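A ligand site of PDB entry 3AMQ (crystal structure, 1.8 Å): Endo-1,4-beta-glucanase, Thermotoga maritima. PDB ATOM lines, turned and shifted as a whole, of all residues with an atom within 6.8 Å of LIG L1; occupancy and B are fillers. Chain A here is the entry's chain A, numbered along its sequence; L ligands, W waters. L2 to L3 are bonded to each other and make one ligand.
An oxygen (O4) of LIG L1 lies within hydrogen-bond range of the side-chain carboxylate of Glu 239 (2.4 Å). An oxygen (O2) of LIG L1 sits at hydrogen-bond distance from the backbone carbonyl oxygen (O) of Thr 153 (2.8 Å). An oxygen (O3) of LIG L1 lies within hydrogen-bond range of the side-chain hydroxyl (OH) of Tyr 188, at 2.9 Å. O6 of LIG L1 is in hydrogen-bond range of O of Arg 68 (2.9 Å). The guanidinium group (NH2) of Arg 68 lies within hydrogen-bond range of an oxygen (O6) of LIG L1, at 3.4 Å. The backbone NH (N) of Gly 155 lies close to an oxygen (O1) of LIG L1, at 3.5 Å. The side-chain sulfur (SD) of Met 144 sits at hydrogen-bond distance from an oxygen (O3) of LIG L1 (3.7 Å). OE1 of Glu 239 lies within hydrogen-bond range of O6 of LG2 L2 (2.8 Å). NH2 of Arg 68 sits at hydrogen-bond distance from O3 of LG2 L2, at 2.8 Å. SD of Met 144 lies within hydrogen-bond range of O1 of LG2 L2 (3.5 Å). An oxygen (O6) of LG2 L2 is in hydrogen-bond range of the indole nitrogen (NE1) of Trp 34, 3.0 Å away. The side-chain carboxylate (OE2) of Glu 124 sits at hydrogen-bond distance from an oxygen (O1) of LG2 L2, at 2.9 Å.
The backbone NH (N) of Glu 239 lies within hydrogen-bond range of the side-chain amide oxygen (OD1) of Asn 120, at 2.8 Å. OH of Tyr 188 is in hydrogen-bond range of N of Gly 155. NE1 of Trp 146 sits at hydrogen-bond distance from SD of Met 144, 3.6 Å away.
Residues that only touch LIG L1: Trp 34, Val 70, Trp 146, Leu 152, Pro 154 and Trp 184. Hydrophobic or aromatic side chains within 4 Å of LIG L1: Trp 34, Val 70, Met 144, Trp 146, Leu 152, Trp 184 and Tyr 188. Within 4 Å of LIG L1: Trp 34, Arg 68, Val 70, Met 144, Trp 146, Leu 152, Thr 153, Pro 154, Gly 155, Trp 184, Tyr 188 and Glu 239. The nearest printed residue that does not touch LIG L1 is Tyr 69 (4.3 Å).
O4 of LIG L1 lies within hydrogen-bond range of O5 of LG2 L2 (2.9 Å).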
ATOM      1  N   TRP A  34     -31.217 -17.827 -17.621  1.00  0.00           N
ATOM      2  CA  TRP A  34     -30.904 -16.648 -18.457  1.00  0.00           C
ATOM      3  C   TRP A  34     -29.957 -16.816 -19.636  1.00  0.00           C
ATOM      4  O   TRP A  34     -30.108 -16.119 -20.629  1.00  0.00           O
ATOM      5  CB  TRP A  34     -30.433 -15.475 -17.567  1.00  0.00           C
ATOM      6  CG  TRP A  34     -29.049 -15.682 -16.979  1.00  0.00           C
ATOM      7  CD1 TRP A  34     -28.719 -16.316 -15.794  1.00  0.00           C
ATOM      8  CD2 TRP A  34     -27.792 -15.202 -17.531  1.00  0.00           C
ATOM      9  NE1 TRP A  34     -27.353 -16.238 -15.576  1.00  0.00           N
ATOM     10  CE2 TRP A  34     -26.771 -15.557 -16.624  1.00  0.00           C
ATOM     11  CE3 TRP A  34     -27.458 -14.512 -18.702  1.00  0.00           C
ATOM     12  CZ2 TRP A  34     -25.405 -15.231 -16.848  1.00  0.00           C
ATOM     13  CZ3 TRP A  34     -26.091 -14.179 -18.933  1.00  0.00           C
ATOM     14  CH2 TRP A  34     -25.088 -14.543 -17.993  1.00  0.00           C
ATOM     15  N   GLU A  67     -19.647 -16.699 -24.146  1.00  0.00           N
ATOM     16  CA  GLU A  67     -18.728 -15.847 -23.406  1.00  0.00           C
ATOM     17  C   GLU A  67     -19.058 -15.671 -21.921  1.00  0.00           C
ATOM     18  O   GLU A  67     -18.151 -15.413 -21.115  1.00  0.00           O
ATOM     19  CB  GLU A  67     -18.700 -14.453 -24.040  1.00  0.00           C
ATOM     20  CG  GLU A  67     -18.286 -14.467 -25.487  1.00  0.00           C
ATOM     21  CD  GLU A  67     -16.854 -14.906 -25.580  1.00  0.00           C
ATOM     22  OE1 GLU A  67     -15.962 -14.048 -25.290  1.00  0.00           O
ATOM     23  OE2 GLU A  67     -16.615 -16.099 -25.911  1.00  0.00           O
ATOM     24  N   ARG A  68     -20.360 -15.755 -21.585  1.00  0.00           N
ATOM     25  CA  ARG A  68     -20.825 -15.570 -20.183  1.00  0.00           C
ATOM     26  C   ARG A  68     -20.536 -16.790 -19.287  1.00  0.00           C
ATOM     27  O   ARG A  68     -20.635 -16.743 -18.041  1.00  0.00           O
ATOM     28  CB  ARG A  68     -22.323 -15.227 -20.155  1.00  0.00           C
ATOM     29  CG  ARG A  68     -22.689 -14.034 -20.990  1.00  0.00           C
ATOM     30  CD  ARG A  68     -21.819 -12.790 -20.657  1.00  0.00           C
ATOM     31  NE  ARG A  68     -21.901 -12.485 -19.229  1.00  0.00           N
ATOM     32  CZ  ARG A  68     -22.954 -11.898 -18.658  1.00  0.00           C
ATOM     33  NH1 ARG A  68     -24.006 -11.534 -19.391  1.00  0.00           N
ATOM     34  NH2 ARG A  68     -22.953 -11.668 -17.361  1.00  0.00           N
ATOM     35  N   TYR A  69     -20.209 -17.896 -19.948  1.00  0.00           N
ATOM     36  CA  TYR A  69     -19.810 -19.119 -19.297  1.00  0.00           C
ATOM     37  C   TYR A  69     -20.927 -19.893 -18.637  1.00  0.00           C
ATOM     38  O   TYR A  69     -21.260 -20.951 -19.158  1.00  0.00           O
ATOM     39  CB  TYR A  69     -18.698 -18.870 -18.268  1.00  0.00           C
ATOM     40  CG  TYR A  69     -18.020 -20.144 -17.845  1.00  0.00           C
ATOM     41  CD1 TYR A  69     -16.898 -20.609 -18.538  1.00  0.00           C
ATOM     42  CD2 TYR A  69     -18.551 -20.970 -16.833  1.00  0.00           C
ATOM     43  CE1 TYR A  69     -16.330 -21.862 -18.256  1.00  0.00           C
ATOM     44  CE2 TYR A  69     -17.995 -22.217 -16.546  1.00  0.00           C
ATOM     45  CZ  TYR A  69     -16.897 -22.651 -17.271  1.00  0.00           C
ATOM     46  OH  TYR A  69     -16.418 -23.918 -17.135  1.00  0.00           O
ATOM     47  N   VAL A  70     -21.520 -19.415 -17.528  1.00  0.00           N
ATOM     48  CA  VAL A  70     -22.594 -20.242 -16.919  1.00  0.00           C
ATOM     49  C   VAL A  70     -23.867 -20.234 -17.794  1.00  0.00           C
ATOM     50  O   VAL A  70     -23.986 -19.433 -18.750  1.00  0.00           O
ATOM     51  CB  VAL A  70     -22.948 -19.776 -15.428  1.00  0.00           C
ATOM     52  CG1 VAL A  70     -21.717 -19.862 -14.547  1.00  0.00           C
ATOM     53  CG2 VAL A  70     -23.519 -18.398 -15.440  1.00  0.00           C
ATOM     54  N   ASN A 120     -22.526 -23.630  -8.448  1.00  0.00           N
ATOM     55  CA  ASN A 120     -22.222 -23.047  -7.136  1.00  0.00           C
ATOM     56  C   ASN A 120     -23.486 -22.839  -6.357  1.00  0.00           C
ATOM     57  O   ASN A 120     -24.602 -23.094  -6.848  1.00  0.00           O
ATOM     58  CB  ASN A 120     -21.449 -21.707  -7.227  1.00  0.00           C
ATOM     59  CG  ASN A 120     -22.212 -20.600  -7.943  1.00  0.00           C
ATOM     60  OD1 ASN A 120     -23.444 -20.540  -7.858  1.00  0.00           O
ATOM     61  ND2 ASN A 120     -21.477 -19.705  -8.641  1.00  0.00           N
ATOM     62  N   ALA A 122     -24.576 -19.597  -4.522  1.00  0.00           N
ATOM     63  CA  ALA A 122     -24.098 -18.239  -4.317  1.00  0.00           C
ATOM     64  C   ALA A 122     -25.207 -17.261  -4.126  1.00  0.00           C
ATOM     65  O   ALA A 122     -26.308 -17.376  -4.684  1.00  0.00           O
ATOM     66  CB  ALA A 122     -23.240 -17.779  -5.482  1.00  0.00           C
ATOM     67  N   GLU A 124     -26.120 -13.035  -4.025  1.00  0.00           N
ATOM     68  CA  GLU A 124     -25.572 -11.829  -4.637  1.00  0.00           C
ATOM     69  C   GLU A 124     -26.453 -10.582  -4.592  1.00  0.00           C
ATOM     70  O   GLU A 124     -27.661 -10.633  -4.304  1.00  0.00           O
ATOM     71  CB  GLU A 124     -25.148 -12.120  -6.078  1.00  0.00           C
ATOM     72  CG  GLU A 124     -26.272 -12.102  -7.062  1.00  0.00           C
ATOM     73  CD  GLU A 124     -25.800 -12.091  -8.545  1.00  0.00           C
ATOM     74  OE1 GLU A 124     -26.635 -11.984  -9.404  1.00  0.00           O
ATOM     75  OE2 GLU A 124     -24.592 -12.194  -8.871  1.00  0.00           O
ATOM     76  N   MET A 144     -20.957 -11.133  -5.054  1.00  0.00           N
ATOM     77  CA  MET A 144     -21.487 -12.477  -4.818  1.00  0.00           C
ATOM     78  C   MET A 144     -20.804 -13.063  -3.605  1.00  0.00           C
ATOM     79  O   MET A 144     -19.639 -12.697  -3.284  1.00  0.00           O
ATOM     80  CB  MET A 144     -21.158 -13.393  -6.019  1.00  0.00           C
ATOM     81  CG  MET A 144     -21.661 -12.850  -7.382  1.00  0.00           C
ATOM     82  SD  MET A 144     -21.537 -14.192  -8.659  1.00  0.00           S
ATOM     83  CE  MET A 144     -23.101 -15.083  -8.192  1.00  0.00           C
ATOM     84  N   TRP A 146     -20.136 -16.939  -2.372  1.00  0.00           N
ATOM     85  CA  TRP A 146     -20.225 -18.345  -2.699  1.00  0.00           C
ATOM     86  C   TRP A 146     -20.003 -19.225  -1.484  1.00  0.00           C
ATOM     87  O   TRP A 146     -18.908 -19.229  -0.942  1.00  0.00           O
ATOM     88  CB  TRP A 146     -19.130 -18.697  -3.718  1.00  0.00           C
ATOM     89  CG  TRP A 146     -19.314 -18.116  -5.134  1.00  0.00           C
ATOM     90  CD1 TRP A 146     -19.851 -16.931  -5.456  1.00  0.00           C
ATOM     91  CD2 TRP A 146     -18.830 -18.696  -6.341  1.00  0.00           C
ATOM     92  NE1 TRP A 146     -19.743 -16.707  -6.835  1.00  0.00           N
ATOM     93  CE2 TRP A 146     -19.111 -17.785  -7.393  1.00  0.00           C
ATOM     94  CE3 TRP A 146     -18.185 -19.882  -6.648  1.00  0.00           C
ATOM     95  CZ2 TRP A 146     -18.755 -18.048  -8.725  1.00  0.00           C
ATOM     96  CZ3 TRP A 146     -17.840 -20.153  -7.975  1.00  0.00           C
ATOM     97  CH2 TRP A 146     -18.119 -19.251  -8.992  1.00  0.00           C
ATOM     98  N   LEU A 152     -16.166 -25.244 -10.628  1.00  0.00           N
ATOM     99  CA  LEU A 152     -16.491 -23.909 -11.116  1.00  0.00           C
ATOM    100  C   LEU A 152     -15.667 -22.900 -10.322  1.00  0.00           C
ATOM    101  O   LEU A 152     -15.580 -22.970  -9.076  1.00  0.00           O
ATOM    102  CB  LEU A 152     -17.982 -23.593 -10.900  1.00  0.00           C
ATOM    103  CG  LEU A 152     -18.442 -22.209 -11.424  1.00  0.00           C
ATOM    104  CD1 LEU A 152     -18.286 -22.194 -12.958  1.00  0.00           C
ATOM    105  CD2 LEU A 152     -19.928 -21.920 -11.099  1.00  0.00           C
ATOM    106  N   THR A 153     -15.079 -21.963 -11.052  1.00  0.00           N
ATOM    107  CA  THR A 153     -14.261 -20.907 -10.453  1.00  0.00           C
ATOM    108  C   THR A 153     -14.901 -19.577 -10.739  1.00  0.00           C
ATOM    109  O   THR A 153     -15.460 -19.386 -11.812  1.00  0.00           O
ATOM    110  CB  THR A 153     -12.864 -20.964 -11.104  1.00  0.00           C
ATOM    111  OG1 THR A 153     -12.346 -22.309 -10.957  1.00  0.00           O
ATOM    112  CG2 THR A 153     -11.917 -19.944 -10.440  1.00  0.00           C
ATOM    113  N   PRO A 154     -14.842 -18.622  -9.794  1.00  0.00           N
ATOM    114  CA  PRO A 154     -15.451 -17.309 -10.030  1.00  0.00           C
ATOM    115  C   PRO A 154     -14.800 -16.626 -11.199  1.00  0.00           C
ATOM    116  O   PRO A 154     -13.704 -17.003 -11.608  1.00  0.00           O
ATOM    117  CB  PRO A 154     -15.210 -16.557  -8.721  1.00  0.00           C
ATOM    118  CG  PRO A 154     -15.108 -17.673  -7.732  1.00  0.00           C
ATOM    119  CD  PRO A 154     -14.275 -18.688  -8.449  1.00  0.00           C
ATOM    120  N   GLY A 155     -15.471 -15.619 -11.777  1.00  0.00           N
ATOM    121  CA  GLY A 155     -14.823 -14.926 -12.887  1.00  0.00           C
ATOM    122  C   GLY A 155     -13.741 -13.977 -12.401  1.00  0.00           C
ATOM    123  O   GLY A 155     -13.589 -13.746 -11.177  1.00  0.00           O
ATOM    124  N   GLY A 156     -12.962 -13.442 -13.324  1.00  0.00           N
ATOM    125  CA  GLY A 156     -11.926 -12.473 -12.949  1.00  0.00           C
ATOM    126  C   GLY A 156     -10.708 -13.163 -12.389  1.00  0.00           C
ATOM    127  O   GLY A 156     -10.462 -14.343 -12.702  1.00  0.00           O
ATOM    128  N   TRP A 184     -15.596  -6.040 -15.939  1.00  0.00           N
ATOM    129  CA  TRP A 184     -16.275  -6.337 -17.189  1.00  0.00           C
ATOM    130  C   TRP A 184     -17.113  -5.121 -17.544  1.00  0.00           C
ATOM    131  O   TRP A 184     -16.613  -3.988 -17.473  1.00  0.00           O
ATOM    132  CB  TRP A 184     -17.188  -7.557 -17.035  1.00  0.00           C
ATOM    133  CG  TRP A 184     -16.500  -8.858 -16.736  1.00  0.00           C
ATOM    134  CD1 TRP A 184     -15.296  -9.310 -17.255  1.00  0.00           C
ATOM    135  CD2 TRP A 184     -17.022  -9.933 -15.934  1.00  0.00           C
ATOM    136  NE1 TRP A 184     -15.041 -10.601 -16.824  1.00  0.00           N
ATOM    137  CE2 TRP A 184     -16.083 -11.007 -16.012  1.00  0.00           C
ATOM    138  CE3 TRP A 184     -18.181 -10.091 -15.155  1.00  0.00           C
ATOM    139  CZ2 TRP A 184     -16.285 -12.215 -15.341  1.00  0.00           C
ATOM    140  CZ3 TRP A 184     -18.381 -11.306 -14.491  1.00  0.00           C
ATOM    141  CH2 TRP A 184     -17.436 -12.350 -14.594  1.00  0.00           C
ATOM    142  N   TRP A 186     -19.366  -4.136 -15.816  1.00  0.00           N
ATOM    143  CA  TRP A 186     -19.615  -3.535 -14.516  1.00  0.00           C
ATOM    144  C   TRP A 186     -18.588  -4.245 -13.711  1.00  0.00           C
ATOM    145  O   TRP A 186     -17.907  -5.134 -14.222  1.00  0.00           O
ATOM    146  CB  TRP A 186     -21.046  -3.838 -14.014  1.00  0.00           C
ATOM    147  CG  TRP A 186     -21.413  -5.308 -14.077  1.00  0.00           C
ATOM    148  CD1 TRP A 186     -21.083  -6.272 -13.184  1.00  0.00           C
ATOM    149  CD2 TRP A 186     -22.135  -5.966 -15.136  1.00  0.00           C
ATOM    150  NE1 TRP A 186     -21.538  -7.501 -13.622  1.00  0.00           N
ATOM    151  CE2 TRP A 186     -22.180  -7.340 -14.825  1.00  0.00           C
ATOM    152  CE3 TRP A 186     -22.731  -5.521 -16.323  1.00  0.00           C
ATOM    153  CZ2 TRP A 186     -22.810  -8.286 -15.656  1.00  0.00           C
ATOM    154  CZ3 TRP A 186     -23.362  -6.438 -17.153  1.00  0.00           C
ATOM    155  CH2 TRP A 186     -23.397  -7.829 -16.797  1.00  0.00           C
ATOM    156  N   TYR A 188     -17.370  -6.917 -11.050  1.00  0.00           N
ATOM    157  CA  TYR A 188     -17.847  -8.154 -10.475  1.00  0.00           C
ATOM    158  C   TYR A 188     -16.890  -8.517  -9.342  1.00  0.00           C
ATOM    159  O   TYR A 188     -15.687  -8.605  -9.560  1.00  0.00           O
ATOM    160  CB  TYR A 188     -17.827  -9.246 -11.578  1.00  0.00           C
ATOM    161  CG  TYR A 188     -17.887 -10.687 -11.115  1.00  0.00           C
ATOM    162  CD1 TYR A 188     -19.097 -11.411 -11.150  1.00  0.00           C
ATOM    163  CD2 TYR A 188     -16.730 -11.367 -10.729  1.00  0.00           C
ATOM    164  CE1 TYR A 188     -19.148 -12.759 -10.810  1.00  0.00           C
ATOM    165  CE2 TYR A 188     -16.768 -12.756 -10.402  1.00  0.00           C
ATOM    166  CZ  TYR A 188     -17.986 -13.423 -10.450  1.00  0.00           C
ATOM    167  OH  TYR A 188     -18.031 -14.767 -10.181  1.00  0.00           O
ATOM    168  N   ALA A 190     -16.536 -11.404  -6.368  1.00  0.00           N
ATOM    169  CA  ALA A 190     -17.088 -12.629  -5.781  1.00  0.00           C
ATOM    170  C   ALA A 190     -16.200 -13.080  -4.612  1.00  0.00           C
ATOM    171  O   ALA A 190     -14.971 -13.265  -4.765  1.00  0.00           O
ATOM    172  CB  ALA A 190     -17.184 -13.753  -6.870  1.00  0.00           C
ATOM    173  N   GLU A 239     -25.709 -20.966  -9.483  1.00  0.00           N
ATOM    174  CA  GLU A 239     -25.335 -20.841 -10.900  1.00  0.00           C
ATOM    175  C   GLU A 239     -24.896 -22.248 -11.373  1.00  0.00           C
ATOM    176  O   GLU A 239     -24.412 -23.068 -10.572  1.00  0.00           O
ATOM    177  CB  GLU A 239     -24.108 -19.926 -11.073  1.00  0.00           C
ATOM    178  CG  GLU A 239     -24.324 -18.534 -10.629  1.00  0.00           C
ATOM    179  CD  GLU A 239     -23.146 -17.649 -11.115  1.00  0.00           C
ATOM    180  OE1 GLU A 239     -23.221 -17.126 -12.247  1.00  0.00           O
ATOM    181  OE2 GLU A 239     -22.158 -17.562 -10.381  1.00  0.00           O
HETATM  182  C1  LIG L   1     -18.386 -17.162 -12.881  1.00  0.00           C
HETATM  183  C2  LIG L   1     -19.880 -16.839 -12.657  1.00  0.00           C
HETATM  184  C3  LIG L   1     -20.369 -15.754 -13.616  1.00  0.00           C
HETATM  185  C4  LIG L   1     -19.832 -15.886 -15.063  1.00  0.00           C
HETATM  186  C5  LIG L   1     -20.155 -14.661 -15.945  1.00  0.00           C
HETATM  187  C6  LIG L   1     -18.022 -17.237 -14.380  1.00  0.00           C
HETATM  188  O1  LIG L   1     -16.660 -17.419 -14.530  1.00  0.00           O
HETATM  189  O2  LIG L   1     -18.070 -18.406 -12.272  1.00  0.00           O
HETATM  190  O3  LIG L   1     -20.096 -16.382 -11.315  1.00  0.00           O
HETATM  191  O4  LIG L   1     -21.779 -15.810 -13.646  1.00  0.00           O
HETATM  192  O5  LIG L   1     -18.399 -16.035 -15.035  1.00  0.00           O
HETATM  193  O6  LIG L   1     -21.549 -14.584 -16.267  1.00  0.00           O
HETATM  194  C1  LG2 L   2     -22.816 -13.374 -12.276  1.00  0.00           C
HETATM  195  C2  LG2 L   2     -22.980 -12.717 -13.646  1.00  0.00           C
HETATM  196  C3  LG2 L   2     -24.372 -12.101 -13.771  1.00  0.00           C
HETATM  197  C4  LG2 L   2     -25.450 -13.159 -13.529  1.00  0.00           C
HETATM  198  C5  LG2 L   2     -25.168 -13.894 -12.224  1.00  0.00           C
HETATM  199  C6  LG2 L   2     -26.080 -15.122 -12.158  1.00  0.00           C
HETATM  200  O1  LG2 L   2     -22.961 -12.379 -11.252  1.00  0.00           O
HETATM  201  O2  LG2 L   2     -22.002 -11.683 -13.767  1.00  0.00           O
HETATM  202  O3  LG2 L   2     -24.509 -11.554 -15.077  1.00  0.00           O
HETATM  203  O4  LG2 L   2     -26.746 -12.549 -13.407  1.00  0.00           O
HETATM  204  O5  LG2 L   2     -23.825 -14.391 -12.109  1.00  0.00           O
HETATM  205  O6  LG2 L   2     -25.636 -16.050 -13.143  1.00  0.00           O
HETATM  206  C1  LG3 L   3     -29.002 -12.350 -14.172  1.00  0.00           C
HETATM  207  C2  LG3 L   3     -29.928 -12.328 -15.386  1.00  0.00           C
HETATM  208  C3  LG3 L   3     -29.461 -11.197 -16.306  1.00  0.00           C
HETATM  209  C4  LG3 L   3     -27.969 -11.316 -16.618  1.00  0.00           C
HETATM  210  C5  LG3 L   3     -27.544 -10.081 -17.409  1.00  0.00           C
HETATM  211  C6  LG3 L   3     -27.544 -12.533 -14.598  1.00  0.00           C
HETATM  212  O1  LG3 L   3     -29.373 -13.406 -13.268  1.00  0.00           O
HETATM  213  O2  LG3 L   3     -31.274 -12.085 -14.958  1.00  0.00           O
HETATM  214  O3  LG3 L   3     -30.164 -11.261 -17.553  1.00  0.00           O
HETATM  215  O4  LG3 L   3     -27.160 -11.431 -15.430  1.00  0.00           O
HETATM  216  O5  LG3 L   3     -26.157 -10.208 -17.754  1.00  0.00           O
HETATM  217  O   HOH W   1     -19.098 -12.409 -18.266  1.00  0.00           O
HETATM  218  O   HOH W   2     -16.403 -15.695 -16.842  1.00  0.00           O
